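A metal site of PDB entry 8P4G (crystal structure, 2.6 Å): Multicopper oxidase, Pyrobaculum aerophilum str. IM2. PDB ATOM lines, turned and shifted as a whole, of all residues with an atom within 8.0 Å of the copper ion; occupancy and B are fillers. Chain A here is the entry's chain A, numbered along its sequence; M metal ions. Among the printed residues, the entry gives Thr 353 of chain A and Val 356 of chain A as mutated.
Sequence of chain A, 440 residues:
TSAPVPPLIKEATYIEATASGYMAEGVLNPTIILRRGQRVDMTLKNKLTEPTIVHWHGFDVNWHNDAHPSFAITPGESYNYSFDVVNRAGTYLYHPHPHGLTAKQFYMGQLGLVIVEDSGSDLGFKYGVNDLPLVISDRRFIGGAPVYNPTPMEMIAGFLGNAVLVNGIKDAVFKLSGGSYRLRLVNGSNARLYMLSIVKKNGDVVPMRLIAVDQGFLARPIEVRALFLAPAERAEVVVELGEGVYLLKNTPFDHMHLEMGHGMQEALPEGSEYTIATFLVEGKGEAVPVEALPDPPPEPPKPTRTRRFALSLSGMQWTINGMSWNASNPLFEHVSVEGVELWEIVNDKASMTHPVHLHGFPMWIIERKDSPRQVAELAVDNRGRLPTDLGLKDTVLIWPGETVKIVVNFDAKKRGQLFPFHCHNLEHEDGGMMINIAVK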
ATOM      1  N   ILE A 156      10.745  -8.290  23.500  1.00  0.00           N
ATOM      2  CA  ILE A 156      11.619  -7.184  23.117  1.00  0.00           C
ATOM      3  C   ILE A 156      11.875  -7.176  21.609  1.00  0.00           C
ATOM      4  O   ILE A 156      11.863  -6.123  20.975  1.00  0.00           O
ATOM      5  CB  ILE A 156      12.944  -7.260  23.903  1.00  0.00           C
ATOM      6  CG1 ILE A 156      12.684  -7.123  25.408  1.00  0.00           C
ATOM      7  CG2 ILE A 156      13.903  -6.187  23.425  1.00  0.00           C
ATOM      8  CD1 ILE A 156      12.275  -5.733  25.824  1.00  0.00           C
ATOM      9  N   ALA A 157      12.103  -8.350  21.025  1.00  0.00           N
ATOM     10  CA  ALA A 157      12.497  -8.440  19.622  1.00  0.00           C
ATOM     11  C   ALA A 157      11.320  -8.634  18.684  1.00  0.00           C
ATOM     12  O   ALA A 157      11.406  -8.247  17.505  1.00  0.00           O
ATOM     13  CB  ALA A 157      13.496  -9.582  19.436  1.00  0.00           C
ATOM     14  N   ALA A 191       5.430  -8.992  13.719  1.00  0.00           N
ATOM     15  CA  ALA A 191       6.734  -8.359  13.726  1.00  0.00           C
ATOM     16  C   ALA A 191       7.584  -8.718  12.503  1.00  0.00           C
ATOM     17  O   ALA A 191       8.560  -8.019  12.204  1.00  0.00           O
ATOM     18  CB  ALA A 191       7.491  -8.737  15.004  1.00  0.00           C
ATOM     19  N   LEU A 311      14.504   6.645  18.723  1.00  0.00           N
ATOM     20  CA  LEU A 311      14.006   5.312  19.019  1.00  0.00           C
ATOM     21  C   LEU A 311      15.127   4.531  19.705  1.00  0.00           C
ATOM     22  O   LEU A 311      16.176   4.278  19.109  1.00  0.00           O
ATOM     23  CB  LEU A 311      13.558   4.599  17.746  1.00  0.00           C
ATOM     24  CG  LEU A 311      12.593   5.383  16.855  1.00  0.00           C
ATOM     25  CD1 LEU A 311      12.235   4.581  15.615  1.00  0.00           C
ATOM     26  CD2 LEU A 311      11.335   5.761  17.621  1.00  0.00           C
ATOM     27  N   TRP A 318      11.146  -0.307  25.284  1.00  0.00           N
ATOM     28  CA  TRP A 318      11.301   0.475  24.067  1.00  0.00           C
ATOM     29  C   TRP A 318      10.717   1.871  24.276  1.00  0.00           C
ATOM     30  O   TRP A 318       9.611   2.015  24.802  1.00  0.00           O
ATOM     31  CB  TRP A 318      10.606  -0.211  22.885  1.00  0.00           C
ATOM     32  CG  TRP A 318      11.380  -1.347  22.312  1.00  0.00           C
ATOM     33  CD1 TRP A 318      11.096  -2.675  22.430  1.00  0.00           C
ATOM     34  CD2 TRP A 318      12.591  -1.260  21.547  1.00  0.00           C
ATOM     35  NE1 TRP A 318      12.047  -3.430  21.768  1.00  0.00           N
ATOM     36  CE2 TRP A 318      12.977  -2.578  21.221  1.00  0.00           C
ATOM     37  CE3 TRP A 318      13.385  -0.197  21.099  1.00  0.00           C
ATOM     38  CZ2 TRP A 318      14.116  -2.855  20.473  1.00  0.00           C
ATOM     39  CZ3 TRP A 318      14.508  -0.476  20.359  1.00  0.00           C
ATOM     40  CH2 TRP A 318      14.867  -1.792  20.045  1.00  0.00           C
ATOM     41  N   ILE A 320      10.292   6.118  22.828  1.00  0.00           N
ATOM     42  CA  ILE A 320      10.300   7.144  21.793  1.00  0.00           C
ATOM     43  C   ILE A 320      10.609   8.459  22.506  1.00  0.00           C
ATOM     44  O   ILE A 320       9.785   8.938  23.306  1.00  0.00           O
ATOM     45  CB  ILE A 320       8.974   7.215  21.032  1.00  0.00           C
ATOM     46  CG1 ILE A 320       8.655   5.863  20.394  1.00  0.00           C
ATOM     47  CG2 ILE A 320       9.018   8.322  19.983  1.00  0.00           C
ATOM     48  CD1 ILE A 320       7.273   5.784  19.772  1.00  0.00           C
ATOM     49  N   ASN A 347      16.646   6.202  14.313  1.00  0.00           N
ATOM     50  CA  ASN A 347      16.762   4.923  14.996  1.00  0.00           C
ATOM     51  C   ASN A 347      18.196   4.717  15.462  1.00  0.00           C
ATOM     52  O   ASN A 347      19.150   5.040  14.752  1.00  0.00           O
ATOM     53  CB  ASN A 347      16.341   3.767  14.090  1.00  0.00           C
ATOM     54  CG  ASN A 347      16.015   2.500  14.854  1.00  0.00           C
ATOM     55  OD1 ASN A 347      15.910   2.516  16.073  1.00  0.00           O
ATOM     56  ND2 ASN A 347      15.851   1.406  14.126  1.00  0.00           N
ATOM     57  N   SER A 351      19.798  -1.024  18.015  1.00  0.00           N
ATOM     58  CA  SER A 351      18.346  -1.165  17.970  1.00  0.00           C
ATOM     59  C   SER A 351      18.004  -2.205  16.920  1.00  0.00           C
ATOM     60  O   SER A 351      18.852  -3.011  16.516  1.00  0.00           O
ATOM     61  CB  SER A 351      17.694   0.197  17.711  1.00  0.00           C
ATOM     62  OG  SER A 351      16.282   0.091  17.656  1.00  0.00           O
ATOM     63  N   MET A 352      16.759  -2.192  16.463  1.00  0.00           N
ATOM     64  CA  MET A 352      16.304  -3.065  15.392  1.00  0.00           C
ATOM     65  C   MET A 352      15.295  -2.298  14.537  1.00  0.00           C
ATOM     66  O   MET A 352      15.045  -1.104  14.758  1.00  0.00           O
ATOM     67  CB  MET A 352      15.697  -4.361  15.927  1.00  0.00           C
ATOM     68  CG  MET A 352      14.594  -4.171  16.952  1.00  0.00           C
ATOM     69  SD  MET A 352      13.858  -5.745  17.417  1.00  0.00           S
ATOM     70  CE  MET A 352      13.250  -6.290  15.823  1.00  0.00           C
ATOM     71  N   THR A 353      14.724  -2.981  13.555  1.00  0.00           N
ATOM     72  CA  THR A 353      13.788  -2.335  12.640  1.00  0.00           C
ATOM     73  C   THR A 353      12.497  -1.974  13.359  1.00  0.00           C
ATOM     74  O   THR A 353      11.976  -2.760  14.161  1.00  0.00           O
ATOM     75  CB  THR A 353      13.501  -3.238  11.443  1.00  0.00           C
ATOM     76  OG1 THR A 353      13.074  -4.527  11.910  1.00  0.00           O
ATOM     77  CG2 THR A 353      14.740  -3.403  10.581  1.00  0.00           C
ATOM     78  N   HIS A 354      11.979  -0.789  13.065  1.00  0.00           N
ATOM     79  CA  HIS A 354      10.745  -0.295  13.681  1.00  0.00           C
ATOM     80  C   HIS A 354       9.789   0.187  12.616  1.00  0.00           C
ATOM     81  O   HIS A 354      10.038   1.249  11.993  1.00  0.00           O
ATOM     82  CB  HIS A 354      11.051   0.828  14.672  1.00  0.00           C
ATOM     83  CG  HIS A 354      11.870   0.403  15.841  1.00  0.00           C
ATOM     84  ND1 HIS A 354      11.408  -0.479  16.802  1.00  0.00           N
ATOM     85  CD2 HIS A 354      13.126   0.738  16.223  1.00  0.00           C
ATOM     86  CE1 HIS A 354      12.353  -0.676  17.707  1.00  0.00           C
ATOM     87  NE2 HIS A 354      13.399   0.053  17.376  1.00  0.00           N
ATOM     88  N   PRO A 355       8.701  -0.535  12.343  1.00  0.00           N
ATOM     89  CA  PRO A 355       7.641   0.034  11.492  1.00  0.00           C
ATOM     90  C   PRO A 355       6.772   1.024  12.246  1.00  0.00           C
ATOM     91  O   PRO A 355       5.726   0.654  12.780  1.00  0.00           O
ATOM     92  CB  PRO A 355       6.845  -1.203  11.055  1.00  0.00           C
ATOM     93  CG  PRO A 355       7.063  -2.182  12.164  1.00  0.00           C
ATOM     94  CD  PRO A 355       8.459  -1.942  12.674  1.00  0.00           C
ATOM     95  N   VAL A 356       7.182   2.293  12.294  1.00  0.00           N
ATOM     96  CA  VAL A 356       6.464   3.280  13.095  1.00  0.00           C
ATOM     97  C   VAL A 356       5.237   3.771  12.327  1.00  0.00           C
ATOM     98  O   VAL A 356       5.245   3.850  11.092  1.00  0.00           O
ATOM     99  CB  VAL A 356       7.383   4.446  13.504  1.00  0.00           C
ATOM    100  CG1 VAL A 356       8.710   3.914  14.052  1.00  0.00           C
ATOM    101  CG2 VAL A 356       7.600   5.413  12.355  1.00  0.00           C
ATOM    102  N   LEU A 397       9.033   2.124   7.588  1.00  0.00           N
ATOM    103  CA  LEU A 397      10.046   1.297   8.245  1.00  0.00           C
ATOM    104  C   LEU A 397      11.334   2.099   8.412  1.00  0.00           C
ATOM    105  O   LEU A 397      11.799   2.749   7.461  1.00  0.00           O
ATOM    106  CB  LEU A 397      10.304   0.033   7.426  1.00  0.00           C
ATOM    107  CG  LEU A 397      11.350  -0.949   7.978  1.00  0.00           C
ATOM    108  CD1 LEU A 397      10.901  -1.512   9.322  1.00  0.00           C
ATOM    109  CD2 LEU A 397      11.596  -2.075   6.980  1.00  0.00           C
ATOM    110  N   ILE A 398      11.903   2.057   9.613  1.00  0.00           N
ATOM    111  CA  ILE A 398      13.153   2.737   9.927  1.00  0.00           C
ATOM    112  C   ILE A 398      14.146   1.687  10.409  1.00  0.00           C
ATOM    113  O   ILE A 398      13.854   0.923  11.339  1.00  0.00           O
ATOM    114  CB  ILE A 398      12.971   3.843  10.972  1.00  0.00           C
ATOM    115  CG1 ILE A 398      12.029   4.944  10.468  1.00  0.00           C
ATOM    116  CG2 ILE A 398      14.307   4.478  11.316  1.00  0.00           C
ATOM    117  CD1 ILE A 398      10.578   4.680  10.725  1.00  0.00           C
ATOM    118  N   HIS A 422       3.161   5.047  17.442  1.00  0.00           N
ATOM    119  CA  HIS A 422       3.756   3.844  18.005  1.00  0.00           C
ATOM    120  C   HIS A 422       4.428   3.043  16.901  1.00  0.00           C
ATOM    121  O   HIS A 422       4.214   3.285  15.711  1.00  0.00           O
ATOM    122  CB  HIS A 422       2.713   2.995  18.714  1.00  0.00           C
ATOM    123  CG  HIS A 422       1.643   2.470  17.804  1.00  0.00           C
ATOM    124  ND1 HIS A 422       1.774   1.293  17.093  1.00  0.00           N
ATOM    125  CD2 HIS A 422       0.419   2.975  17.481  1.00  0.00           C
ATOM    126  CE1 HIS A 422       0.682   1.091  16.380  1.00  0.00           C
ATOM    127  NE2 HIS A 422      -0.153   2.089  16.596  1.00  0.00           N
ATOM    128  N   CYS A 423       5.240   2.084  17.321  1.00  0.00           N
ATOM    129  CA  CYS A 423       5.789   1.095  16.404  1.00  0.00           C
ATOM    130  C   CYS A 423       4.761   0.000  16.180  1.00  0.00           C
ATOM    131  O   CYS A 423       4.066  -0.417  17.119  1.00  0.00           O
ATOM    132  CB  CYS A 423       7.083   0.513  16.959  1.00  0.00           C
ATOM    133  SG  CYS A 423       7.755  -0.830  15.984  1.00  0.00           S
ATOM    134  N   HIS A 424       4.651  -0.467  14.941  1.00  0.00           N
ATOM    135  CA  HIS A 424       3.659  -1.486  14.616  1.00  0.00           C
ATOM    136  C   HIS A 424       4.200  -2.895  14.770  1.00  0.00           C
ATOM    137  O   HIS A 424       3.530  -3.857  14.382  1.00  0.00           O
ATOM    138  CB  HIS A 424       3.116  -1.272  13.204  1.00  0.00           C
ATOM    139  CG  HIS A 424       1.625  -1.382  13.116  1.00  0.00           C
ATOM    140  ND1 HIS A 424       0.952  -2.574  13.216  1.00  0.00           N
ATOM    141  CD2 HIS A 424       0.681  -0.428  12.953  1.00  0.00           C
ATOM    142  CE1 HIS A 424      -0.350  -2.358  13.125  1.00  0.00           C
ATOM    143  NE2 HIS A 424      -0.539  -1.062  12.961  1.00  0.00           N
ATOM    144  N   ASN A 425       5.397  -3.045  15.332  1.00  0.00           N
ATOM    145  CA  ASN A 425       5.819  -4.308  15.927  1.00  0.00           C
ATOM    146  C   ASN A 425       4.958  -4.532  17.158  1.00  0.00           C
ATOM    147  O   ASN A 425       5.143  -3.860  18.180  1.00  0.00           O
ATOM    148  CB  ASN A 425       7.307  -4.263  16.265  1.00  0.00           C
ATOM    149  CG  ASN A 425       7.841  -5.585  16.814  1.00  0.00           C
ATOM    150  OD1 ASN A 425       7.170  -6.275  17.595  1.00  0.00           O
ATOM    151  ND2 ASN A 425       9.054  -5.940  16.420  1.00  0.00           N
ATOM    152  N   LEU A 426       4.014  -5.461  17.071  1.00  0.00           N
ATOM    153  CA  LEU A 426       2.982  -5.567  18.103  1.00  0.00           C
ATOM    154  C   LEU A 426       3.557  -5.949  19.458  1.00  0.00           C
ATOM    155  O   LEU A 426       2.985  -5.604  20.496  1.00  0.00           O
ATOM    156  CB  LEU A 426       1.912  -6.561  17.659  1.00  0.00           C
ATOM    157  CG  LEU A 426       1.193  -6.133  16.388  1.00  0.00           C
ATOM    158  CD1 LEU A 426       0.016  -7.038  16.113  1.00  0.00           C
ATOM    159  CD2 LEU A 426       0.747  -4.675  16.488  1.00  0.00           C
ATOM    160  N   GLU A 427       4.694  -6.660  19.482  1.00  0.00           N
ATOM    161  CA  GLU A 427       5.366  -6.900  20.755  1.00  0.00           C
ATOM    162  C   GLU A 427       5.934  -5.605  21.323  1.00  0.00           C
ATOM    163  O   GLU A 427       5.890  -5.394  22.542  1.00  0.00           O
ATOM    164  CB  GLU A 427       6.462  -7.951  20.580  1.00  0.00           C
ATOM    165  CG  GLU A 427       5.955  -9.388  20.589  1.00  0.00           C
ATOM    166  CD  GLU A 427       5.105  -9.710  19.387  1.00  0.00           C
ATOM    167  OE1 GLU A 427       5.547  -9.428  18.251  1.00  0.00           O
ATOM    168  OE2 GLU A 427       3.987 -10.234  19.576  1.00  0.00           O
ATOM    169  N   HIS A 428       6.475  -4.740  20.457  1.00  0.00           N
ATOM    170  CA  HIS A 428       6.976  -3.455  20.931  1.00  0.00           C
ATOM    171  C   HIS A 428       5.856  -2.559  21.410  1.00  0.00           C
ATOM    172  O   HIS A 428       5.985  -1.893  22.449  1.00  0.00           O
ATOM    173  CB  HIS A 428       7.768  -2.759  19.813  1.00  0.00           C
ATOM    174  CG  HIS A 428       8.996  -3.494  19.381  1.00  0.00           C
ATOM    175  ND1 HIS A 428       9.813  -3.044  18.370  1.00  0.00           N
ATOM    176  CD2 HIS A 428       9.541  -4.651  19.827  1.00  0.00           C
ATOM    177  CE1 HIS A 428      10.809  -3.894  18.199  1.00  0.00           C
ATOM    178  NE2 HIS A 428      10.671  -4.870  19.069  1.00  0.00           N
ATOM    179  N   GLU A 429       4.734  -2.538  20.693  1.00  0.00           N
ATOM    180  CA  GLU A 429       3.608  -1.702  21.080  1.00  0.00           C
ATOM    181  C   GLU A 429       2.992  -2.162  22.395  1.00  0.00           C
ATOM    182  O   GLU A 429       2.740  -1.352  23.295  1.00  0.00           O
ATOM    183  CB  GLU A 429       2.550  -1.690  19.982  1.00  0.00           C
ATOM    184  CG  GLU A 429       1.363  -0.804  20.313  1.00  0.00           C
ATOM    185  CD  GLU A 429       0.159  -1.105  19.455  1.00  0.00           C
ATOM    186  OE1 GLU A 429       0.352  -1.506  18.287  1.00  0.00           O
ATOM    187  OE2 GLU A 429      -0.973  -0.945  19.946  1.00  0.00           O
ATOM    188  N   MET A 433       5.779   0.816  23.589  1.00  0.00           N
ATOM    189  CA  MET A 433       6.385   1.745  22.624  1.00  0.00           C
ATOM    190  C   MET A 433       5.268   2.469  21.881  1.00  0.00           C
ATOM    191  O   MET A 433       5.000   2.259  20.699  1.00  0.00           O
ATOM    192  CB  MET A 433       7.315   1.001  21.668  1.00  0.00           C
ATOM    193  CG  MET A 433       8.213   1.941  20.864  1.00  0.00           C
ATOM    194  SD  MET A 433       9.428   1.092  19.842  1.00  0.00           S
ATOM    195  CE  MET A 433      10.264   2.479  19.085  1.00  0.00           C
HETATM  196 CU    CU M   1       9.432  -1.262  17.011  1.00  0.00          CU
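A ring nitrogen (NE2) of His 428 lies close to the side-chain sulfur of Met 352 (3.7 Å).
The backbone NH (N) of Cys 423 lies within hydrogen-bond range of the backbone carbonyl oxygen (O) of Met 433 (3.4 Å).
A ring nitrogen (NE2) of His 428 sits close to the side-chain amide nitrogen of Asn 425, at 3.3 Å.
A ring nitrogen (NE2) of His 354 sits at hydrogen-bond distance from the side-chain hydroxyl (OG) of Ser 351, at 2.9 Å.
The backbone NH of His 354 lies within hydrogen-bond range of the backbone carbonyl oxygen of Ile 398, 3.1 Å away.
O of His 428 lies within hydrogen-bond range of N of Met 433 (2.9 Å).
NE2 of His 428 sits at hydrogen-bond distance from NE1 of Trp 318.
The side-chain amide oxygen of Asn 425 is in hydrogen-bond range of the backbone NH of Glu 427, 3.1 Å away.
Asn 425 touches the copper ion.
SD of Met 433 touches the copper ion, 3.7 Å away.
Five residues have an atom within 4 Å of the copper ion: His 354, Cys 423, Asn 425, His 428 and Met 433.
The copper ion is bound by SG of Cys 423 (2.0 Å), ND1 of His 354 (2.1 Å) and ND1 of His 428 (2.3 Å).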
